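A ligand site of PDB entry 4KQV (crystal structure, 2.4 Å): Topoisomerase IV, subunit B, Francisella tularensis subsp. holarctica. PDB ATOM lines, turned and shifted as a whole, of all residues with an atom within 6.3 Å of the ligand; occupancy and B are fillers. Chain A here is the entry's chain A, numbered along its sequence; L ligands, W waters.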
ATOM      1  N   GLU A  37      -1.296  22.688 -22.989  1.00  0.00           N
ATOM      2  CA  GLU A  37      -0.603  23.980 -23.109  1.00  0.00           C
ATOM      3  C   GLU A  37       0.106  24.355 -21.827  1.00  0.00           C
ATOM      4  O   GLU A  37       1.262  24.783 -21.865  1.00  0.00           O
ATOM      5  CB  GLU A  37      -1.535  25.119 -23.515  1.00  0.00           C
ATOM      6  CG  GLU A  37      -1.616  25.411 -25.001  1.00  0.00           C
ATOM      7  CD  GLU A  37      -0.264  25.594 -25.678  1.00  0.00           C
ATOM      8  OE1 GLU A  37       0.034  24.791 -26.587  1.00  0.00           O
ATOM      9  OE2 GLU A  37       0.497  26.517 -25.309  1.00  0.00           O
ATOM     10  N   ILE A  38      -0.577  24.179 -20.689  1.00  0.00           N
ATOM     11  CA  ILE A  38       0.026  24.518 -19.403  1.00  0.00           C
ATOM     12  C   ILE A  38       1.178  23.584 -19.043  1.00  0.00           C
ATOM     13  O   ILE A  38       2.230  24.053 -18.611  1.00  0.00           O
ATOM     14  CB  ILE A  38      -1.020  24.614 -18.262  1.00  0.00           C
ATOM     15  CG1 ILE A  38      -2.159  25.546 -18.675  1.00  0.00           C
ATOM     16  CG2 ILE A  38      -0.363  25.082 -16.982  1.00  0.00           C
ATOM     17  CD1 ILE A  38      -1.775  27.018 -18.705  1.00  0.00           C
ATOM     18  N   ILE A  39       0.984  22.278 -19.179  1.00  0.00           N
ATOM     19  CA  ILE A  39       2.092  21.307 -18.973  1.00  0.00           C
ATOM     20  C   ILE A  39       3.331  21.694 -19.814  1.00  0.00           C
ATOM     21  O   ILE A  39       4.423  21.861 -19.259  1.00  0.00           O
ATOM     22  CB  ILE A  39       1.644  19.834 -19.218  1.00  0.00           C
ATOM     23  CG1 ILE A  39       0.596  19.408 -18.184  1.00  0.00           C
ATOM     24  CG2 ILE A  39       2.842  18.874 -19.200  1.00  0.00           C
ATOM     25  CD1 ILE A  39      -0.135  18.123 -18.509  1.00  0.00           C
ATOM     26  N   ASN A  41       4.522  24.456 -20.943  1.00  0.00           N
ATOM     27  CA  ASN A  41       5.265  25.588 -20.435  1.00  0.00           C
ATOM     28  C   ASN A  41       6.103  25.189 -19.221  1.00  0.00           C
ATOM     29  O   ASN A  41       7.292  25.565 -19.073  1.00  0.00           O
ATOM     30  CB  ASN A  41       4.293  26.725 -20.055  1.00  0.00           C
ATOM     31  CG  ASN A  41       3.810  27.476 -21.265  1.00  0.00           C
ATOM     32  OD1 ASN A  41       4.332  28.533 -21.587  1.00  0.00           O
ATOM     33  ND2 ASN A  41       2.841  26.920 -21.980  1.00  0.00           N
ATOM     34  N   SER A  42       5.457  24.435 -18.339  1.00  0.00           N
ATOM     35  CA  SER A  42       6.095  23.938 -17.151  1.00  0.00           C
ATOM     36  C   SER A  42       7.204  22.927 -17.562  1.00  0.00           C
ATOM     37  O   SER A  42       8.275  22.873 -16.936  1.00  0.00           O
ATOM     38  CB  SER A  42       5.019  23.330 -16.244  1.00  0.00           C
ATOM     39  OG  SER A  42       5.580  22.793 -15.088  1.00  0.00           O
ATOM     40  N   ASP A  44       9.016  23.230 -20.364  1.00  0.00           N
ATOM     41  CA  ASP A  44      10.116  24.102 -20.788  1.00  0.00           C
ATOM     42  C   ASP A  44      10.991  24.567 -19.612  1.00  0.00           C
ATOM     43  O   ASP A  44      12.189  24.743 -19.759  1.00  0.00           O
ATOM     44  CB  ASP A  44       9.616  25.289 -21.595  1.00  0.00           C
ATOM     45  CG  ASP A  44       9.468  24.973 -23.078  1.00  0.00           C
ATOM     46  OD1 ASP A  44      10.389  24.331 -23.645  1.00  0.00           O
ATOM     47  OD2 ASP A  44       8.444  25.367 -23.680  1.00  0.00           O
ATOM     48  N   GLU A  45      10.381  24.765 -18.451  1.00  0.00           N
ATOM     49  CA  GLU A  45      11.121  25.128 -17.262  1.00  0.00           C
ATOM     50  C   GLU A  45      11.886  23.932 -16.659  1.00  0.00           C
ATOM     51  O   GLU A  45      12.968  24.126 -16.104  1.00  0.00           O
ATOM     52  CB  GLU A  45      10.204  25.825 -16.241  1.00  0.00           C
ATOM     53  CG  GLU A  45      10.935  26.490 -15.072  1.00  0.00           C
ATOM     54  CD  GLU A  45      11.804  27.696 -15.442  1.00  0.00           C
ATOM     55  OE1 GLU A  45      12.388  28.266 -14.504  1.00  0.00           O
ATOM     56  OE2 GLU A  45      11.901  28.090 -16.635  1.00  0.00           O
ATOM     57  N   ILE A  54       6.262  18.707 -11.313  1.00  0.00           N
ATOM     58  CA  ILE A  54       5.026  19.175 -11.917  1.00  0.00           C
ATOM     59  C   ILE A  54       3.870  18.476 -11.208  1.00  0.00           C
ATOM     60  O   ILE A  54       3.744  17.246 -11.284  1.00  0.00           O
ATOM     61  CB  ILE A  54       4.961  18.892 -13.427  1.00  0.00           C
ATOM     62  CG1 ILE A  54       6.142  19.524 -14.188  1.00  0.00           C
ATOM     63  CG2 ILE A  54       3.632  19.406 -14.001  1.00  0.00           C
ATOM     64  CD1 ILE A  54       6.200  19.146 -15.669  1.00  0.00           C
ATOM     65  N   VAL A  66      -2.140  23.297 -12.341  1.00  0.00           N
ATOM     66  CA  VAL A  66      -0.796  22.781 -12.611  1.00  0.00           C
ATOM     67  C   VAL A  66       0.244  23.641 -11.884  1.00  0.00           C
ATOM     68  O   VAL A  66       0.229  24.872 -12.011  1.00  0.00           O
ATOM     69  CB  VAL A  66      -0.469  22.766 -14.139  1.00  0.00           C
ATOM     70  CG1 VAL A  66       0.850  22.056 -14.385  1.00  0.00           C
ATOM     71  CG2 VAL A  66      -1.590  22.115 -14.968  1.00  0.00           C
ATOM     72  N   ALA A  67       1.147  23.016 -11.139  1.00  0.00           N
ATOM     73  CA  ALA A  67       2.176  23.742 -10.407  1.00  0.00           C
ATOM     74  C   ALA A  67       3.582  23.207 -10.643  1.00  0.00           C
ATOM     75  O   ALA A  67       3.803  22.004 -10.730  1.00  0.00           O
ATOM     76  CB  ALA A  67       1.871  23.713  -8.902  1.00  0.00           C
ATOM     77  N   ASP A  68       4.545  24.113 -10.730  1.00  0.00           N
ATOM     78  CA  ASP A  68       5.934  23.680 -10.801  1.00  0.00           C
ATOM     79  C   ASP A  68       6.803  24.385  -9.741  1.00  0.00           C
ATOM     80  O   ASP A  68       6.321  25.292  -9.055  1.00  0.00           O
ATOM     81  CB  ASP A  68       6.484  23.820 -12.224  1.00  0.00           C
ATOM     82  CG  ASP A  68       6.649  25.263 -12.640  1.00  0.00           C
ATOM     83  OD1 ASP A  68       7.303  26.012 -11.887  1.00  0.00           O
ATOM     84  OD2 ASP A  68       6.121  25.655 -13.700  1.00  0.00           O
ATOM     85  N   GLY A  70       9.826  25.764 -10.561  1.00  0.00           N
ATOM     86  CA  GLY A  70      10.760  26.530 -11.400  1.00  0.00           C
ATOM     87  C   GLY A  70      10.957  27.949 -10.914  1.00  0.00           C
ATOM     88  O   GLY A  70      10.534  28.278  -9.803  1.00  0.00           O
ATOM     89  N   ARG A  71      11.573  28.792 -11.735  1.00  0.00           N
ATOM     90  CA  ARG A  71      11.968  30.154 -11.294  1.00  0.00           C
ATOM     91  C   ARG A  71      10.784  31.064 -11.029  1.00  0.00           C
ATOM     92  O   ARG A  71      10.930  32.077 -10.340  1.00  0.00           O
ATOM     93  CB  ARG A  71      12.929  30.829 -12.281  1.00  0.00           C
ATOM     94  CG  ARG A  71      14.280  30.135 -12.436  1.00  0.00           C
ATOM     95  CD  ARG A  71      14.990  30.588 -13.705  1.00  0.00           C
ATOM     96  NE  ARG A  71      14.348  30.111 -14.928  1.00  0.00           N
ATOM     97  CZ  ARG A  71      14.828  30.278 -16.159  1.00  0.00           C
ATOM     98  NH1 ARG A  71      15.968  30.926 -16.358  1.00  0.00           N
ATOM     99  NH2 ARG A  71      14.170  29.814 -17.202  1.00  0.00           N
ATOM    100  N   GLY A  72       9.625  30.716 -11.583  1.00  0.00           N
ATOM    101  CA  GLY A  72       8.433  31.551 -11.517  1.00  0.00           C
ATOM    102  C   GLY A  72       8.327  32.449 -12.742  1.00  0.00           C
ATOM    103  O   GLY A  72       9.331  33.075 -13.139  1.00  0.00           O
ATOM    104  N   MET A  73       7.134  32.491 -13.335  1.00  0.00           N
ATOM    105  CA  MET A  73       6.853  33.349 -14.491  1.00  0.00           C
ATOM    106  C   MET A  73       7.193  34.802 -14.155  1.00  0.00           C
ATOM    107  O   MET A  73       6.747  35.340 -13.136  1.00  0.00           O
ATOM    108  CB  MET A  73       5.389  33.206 -14.939  1.00  0.00           C
ATOM    109  CG  MET A  73       4.925  34.228 -15.973  1.00  0.00           C
ATOM    110  SD  MET A  73       5.661  34.034 -17.622  1.00  0.00           S
ATOM    111  CE  MET A  73       5.531  35.705 -18.233  1.00  0.00           C
ATOM    112  N   PRO A  74       8.018  35.446 -15.004  1.00  0.00           N
ATOM    113  CA  PRO A  74       8.474  36.809 -14.686  1.00  0.00           C
ATOM    114  C   PRO A  74       7.319  37.790 -14.522  1.00  0.00           C
ATOM    115  O   PRO A  74       6.329  37.661 -15.225  1.00  0.00           O
ATOM    116  CB  PRO A  74       9.313  37.200 -15.899  1.00  0.00           C
ATOM    117  CG  PRO A  74       9.766  35.901 -16.457  1.00  0.00           C
ATOM    118  CD  PRO A  74       8.570  35.000 -16.301  1.00  0.00           C
ATOM    119  N   ILE A  89       1.645  37.851 -21.091  1.00  0.00           N
ATOM    120  CA  ILE A  89       1.601  36.522 -21.699  1.00  0.00           C
ATOM    121  C   ILE A  89       0.186  35.919 -21.632  1.00  0.00           C
ATOM    122  O   ILE A  89      -0.209  35.161 -22.524  1.00  0.00           O
ATOM    123  CB  ILE A  89       2.716  35.598 -21.147  1.00  0.00           C
ATOM    124  CG1 ILE A  89       3.172  34.619 -22.246  1.00  0.00           C
ATOM    125  CG2 ILE A  89       2.307  34.942 -19.835  1.00  0.00           C
ATOM    126  CD1 ILE A  89       4.125  33.520 -21.784  1.00  0.00           C
ATOM    127  N   MET A  90      -0.589  36.300 -20.622  1.00  0.00           N
ATOM    128  CA  MET A  90      -1.931  35.744 -20.449  1.00  0.00           C
ATOM    129  C   MET A  90      -3.002  36.367 -21.340  1.00  0.00           C
ATOM    130  O   MET A  90      -4.028  35.734 -21.600  1.00  0.00           O
ATOM    131  CB  MET A  90      -2.383  35.845 -18.995  1.00  0.00           C
ATOM    132  CG  MET A  90      -1.832  34.757 -18.083  1.00  0.00           C
ATOM    133  SD  MET A  90      -2.295  33.133 -18.729  1.00  0.00           S
ATOM    134  CE  MET A  90      -1.349  32.035 -17.671  1.00  0.00           C
ATOM    135  N   VAL A 115      -0.138  30.164 -23.537  1.00  0.00           N
ATOM    136  CA  VAL A 115      -1.098  30.057 -22.433  1.00  0.00           C
ATOM    137  C   VAL A 115      -2.299  31.015 -22.556  1.00  0.00           C
ATOM    138  O   VAL A 115      -3.329  30.786 -21.938  1.00  0.00           O
ATOM    139  CB  VAL A 115      -0.403  30.215 -21.041  1.00  0.00           C
ATOM    140  CG1 VAL A 115       0.592  29.091 -20.804  1.00  0.00           C
ATOM    141  CG2 VAL A 115       0.278  31.575 -20.891  1.00  0.00           C
ATOM    142  N   ARG A 131       8.474  34.165  -6.503  1.00  0.00           N
ATOM    143  CA  ARG A 131       9.836  34.587  -6.881  1.00  0.00           C
ATOM    144  C   ARG A 131      10.307  35.631  -5.902  1.00  0.00           C
ATOM    145  O   ARG A 131       9.489  36.406  -5.359  1.00  0.00           O
ATOM    146  CB  ARG A 131       9.895  35.306  -8.233  1.00  0.00           C
ATOM    147  CG  ARG A 131       9.336  34.657  -9.470  1.00  0.00           C
ATOM    148  CD  ARG A 131       9.240  35.713 -10.584  1.00  0.00           C
ATOM    149  NE  ARG A 131      10.511  36.391 -10.840  1.00  0.00           N
ATOM    150  CZ  ARG A 131      11.441  35.970 -11.697  1.00  0.00           C
ATOM    151  NH1 ARG A 131      11.273  34.849 -12.382  1.00  0.00           N
ATOM    152  NH2 ARG A 131      12.565  36.658 -11.862  1.00  0.00           N
ATOM    153  N   GLY A 161       8.369  29.211  -7.952  1.00  0.00           N
ATOM    154  CA  GLY A 161       7.398  28.446  -8.742  1.00  0.00           C
ATOM    155  C   GLY A 161       6.236  29.197  -9.362  1.00  0.00           C
ATOM    156  O   GLY A 161       6.003  30.375  -9.078  1.00  0.00           O
ATOM    157  N   THR A 162       5.542  28.491 -10.248  1.00  0.00           N
ATOM    158  CA  THR A 162       4.396  29.001 -10.965  1.00  0.00           C
ATOM    159  C   THR A 162       3.259  28.003 -10.762  1.00  0.00           C
ATOM    160  O   THR A 162       3.470  26.788 -10.865  1.00  0.00           O
ATOM    161  CB  THR A 162       4.660  29.097 -12.489  1.00  0.00           C
ATOM    162  OG1 THR A 162       5.865  29.825 -12.756  1.00  0.00           O
ATOM    163  CG2 THR A 162       3.498  29.754 -13.199  1.00  0.00           C
ATOM    164  N   LYS A 163       2.072  28.522 -10.496  1.00  0.00           N
ATOM    165  CA  LYS A 163       0.901  27.694 -10.273  1.00  0.00           C
ATOM    166  C   LYS A 163      -0.273  28.361 -10.972  1.00  0.00           C
ATOM    167  O   LYS A 163      -0.542  29.554 -10.756  1.00  0.00           O
ATOM    168  CB  LYS A 163       0.621  27.582  -8.772  1.00  0.00           C
ATOM    169  CG  LYS A 163      -0.506  26.629  -8.408  1.00  0.00           C
ATOM    170  CD  LYS A 163      -0.284  26.088  -7.012  1.00  0.00           C
ATOM    171  CE  LYS A 163      -1.077  26.852  -5.966  1.00  0.00           C
ATOM    172  NZ  LYS A 163      -0.780  26.241  -4.634  1.00  0.00           N
ATOM    173  N   ILE A 164      -0.954  27.593 -11.821  1.00  0.00           N
ATOM    174  CA  ILE A 164      -2.038  28.103 -12.645  1.00  0.00           C
ATOM    175  C   ILE A 164      -3.241  27.240 -12.374  1.00  0.00           C
ATOM    176  O   ILE A 164      -3.152  26.021 -12.485  1.00  0.00           O
ATOM    177  CB  ILE A 164      -1.732  27.988 -14.158  1.00  0.00           C
ATOM    178  CG1 ILE A 164      -0.435  28.720 -14.554  1.00  0.00           C
ATOM    179  CG2 ILE A 164      -2.935  28.412 -14.998  1.00  0.00           C
ATOM    180  CD1 ILE A 164      -0.370  30.204 -14.252  1.00  0.00           C
HETATM  181  F1  LIG L   1       1.734  28.844 -18.100  1.00  0.00           F
HETATM  182  C1  LIG L   1       2.795  28.589 -17.341  1.00  0.00           C
HETATM  183  C2  LIG L   1       2.644  27.628 -16.356  1.00  0.00           C
HETATM  184  C3  LIG L   1       3.986  29.304 -17.562  1.00  0.00           C
HETATM  185  C4  LIG L   1       5.056  29.008 -16.755  1.00  0.00           C
HETATM  186  C5  LIG L   1       6.438  29.500 -16.691  1.00  0.00           C
HETATM  187  C6  LIG L   1       7.219  30.542 -17.407  1.00  0.00           C
HETATM  188  N1  LIG L   1       6.827  31.262 -18.561  1.00  0.00           N
HETATM  189  C7  LIG L   1       7.618  32.349 -19.116  1.00  0.00           C
HETATM  190  C8  LIG L   1       7.541  32.031 -20.607  1.00  0.00           C
HETATM  191  C9  LIG L   1       8.827  31.395 -21.126  1.00  0.00           C
HETATM  192  C10 LIG L   1       8.458  30.033 -21.712  1.00  0.00           C
HETATM  193  N2  LIG L   1       7.054  29.837 -21.392  1.00  0.00           N
HETATM  194  C11 LIG L   1       6.414  31.022 -20.814  1.00  0.00           C
HETATM  195  C12 LIG L   1       5.775  30.761 -19.449  1.00  0.00           C
HETATM  196  N3  LIG L   1       8.511  30.675 -16.966  1.00  0.00           N
HETATM  197  C13 LIG L   1       9.038  29.970 -15.937  1.00  0.00           C
HETATM  198  N4  LIG L   1       8.355  29.021 -15.250  1.00  0.00           N
HETATM  199  C14 LIG L   1       7.070  28.763 -15.572  1.00  0.00           C
HETATM  200  N5  LIG L   1       6.160  27.909 -15.060  1.00  0.00           N
HETATM  201  C15 LIG L   1       4.963  27.980 -15.701  1.00  0.00           C
HETATM  202  C16 LIG L   1       3.694  27.278 -15.525  1.00  0.00           C
HETATM  203  N6  LIG L   1       3.599  26.355 -14.531  1.00  0.00           N
HETATM  204  C17 LIG L   1       2.494  25.420 -14.520  1.00  0.00           C
HETATM  205  O1  LIG L   1      10.312  30.193 -15.579  1.00  0.00           O
HETATM  206  C18 LIG L   1      11.071  31.206 -16.137  1.00  0.00           C
HETATM  207  C19 LIG L   1      11.557  32.230 -15.330  1.00  0.00           C
HETATM  208  N7  LIG L   1      12.317  33.189 -15.892  1.00  0.00           N
HETATM  209  C20 LIG L   1      12.597  33.166 -17.222  1.00  0.00           C
HETATM  210  C21 LIG L   1      13.438  34.257 -17.831  1.00  0.00           C
HETATM  211  N8  LIG L   1      12.124  32.177 -18.013  1.00  0.00           N
HETATM  212  C22 LIG L   1      11.389  31.197 -17.491  1.00  0.00           C
HETATM  213  O   HOH W   1       8.021  28.434 -12.624  1.00  0.00           O
HETATM  214  O   HOH W   2      13.591  34.794 -13.985  1.00  0.00           O
HETATM  215  O   HOH W   3      10.867  28.128 -18.983  1.00  0.00           O
HETATM  216  O   HOH W   4       6.637  27.627 -23.397  1.00  0.00           O
HETATM  217  O   HOH W   5       8.267  28.110 -19.277  1.00  0.00           O
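The side-chain carboxylate of Asp 68 lies close to the side-chain hydroxyl of Ser 42, at 3.2 Å. O of Arg 71 lies close to NH1 of Arg 131 (3.5 Å). The backbone NH (N) of Asp 68 lies within hydrogen-bond range of the backbone carbonyl oxygen (O) of Thr 162 (2.9 Å). The backbone NH (N) of Gly 70 sits at hydrogen-bond distance from the side-chain carboxylate (OD1) of Asp 68 (2.9 Å). The backbone NH of Met 73 sits at hydrogen-bond distance from the side-chain hydroxyl of Thr 162 (3.0 Å). O of Ile 164 is in hydrogen-bond range of N of Val 66. OE1 of Glu 45 is in salt-bridge range of NE of Arg 71, at 2.7 Å. O of Glu 37 sits at hydrogen-bond distance from ND2 of Asn 41, 2.7 Å away.
The side-chain amide oxygen (OD1) of Asn 41 lies within hydrogen-bond range of a nitrogen (N2) of the ligand, 3.0 Å away. The side-chain carboxylate (OD2) of Asp 68 sits at hydrogen-bond distance from a nitrogen (N5) of the ligand (2.6 Å). NH2 of Arg 71 lies close to N8 of the ligand. A nitrogen (N5) of the ligand sits at hydrogen-bond distance from the side-chain hydroxyl of Thr 162.
OE2 of Glu 45 sits close to O1 of the ligand, 2.8 Å away. A nitrogen (N1) of the ligand sits close to the side-chain sulfur (SD) of Met 73 (3.2 Å). Ile 38 touches the ligand (CG2 to C17, 3.8 Å). CB of Ser 42 touches C17 of the ligand, 3.7 Å away. O of Val 66 touches C17 of the ligand, 3.4 Å away. O of Gly 72 touches C19 of the ligand, 3.2 Å away. Pro 74 touches the ligand (CG to N7, 3.8 Å). Ile 89 touches the ligand. Val 115 touches the ligand (CG1 to F1, 2.9 Å). Arg 131 touches the ligand. Ile 164 touches the ligand (CG1 to C2, 3.7 Å). The nearest printed residue that does not touch the ligand is Ala 67 (4.4 Å).
Water W1 lies within hydrogen-bond range of OG1 of Thr 162 (2.6 Å), OD1 of Asp 68 (2.6 Å), N4 of the ligand (2.7 Å) and N of Gly 72 (3.0 Å). Water W2 bridges N7 of the ligand (2.8 Å) and NH1 of Arg 131 (2.8 Å). Water W5 lies within hydrogen-bond range of O of Asn 41 (2.7 Å) and N2 of the ligand (3.0 Å). Water W4 lies within hydrogen-bond range of OD2 of Asp 44, N2 of the ligand and OD1 of Asn 41.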
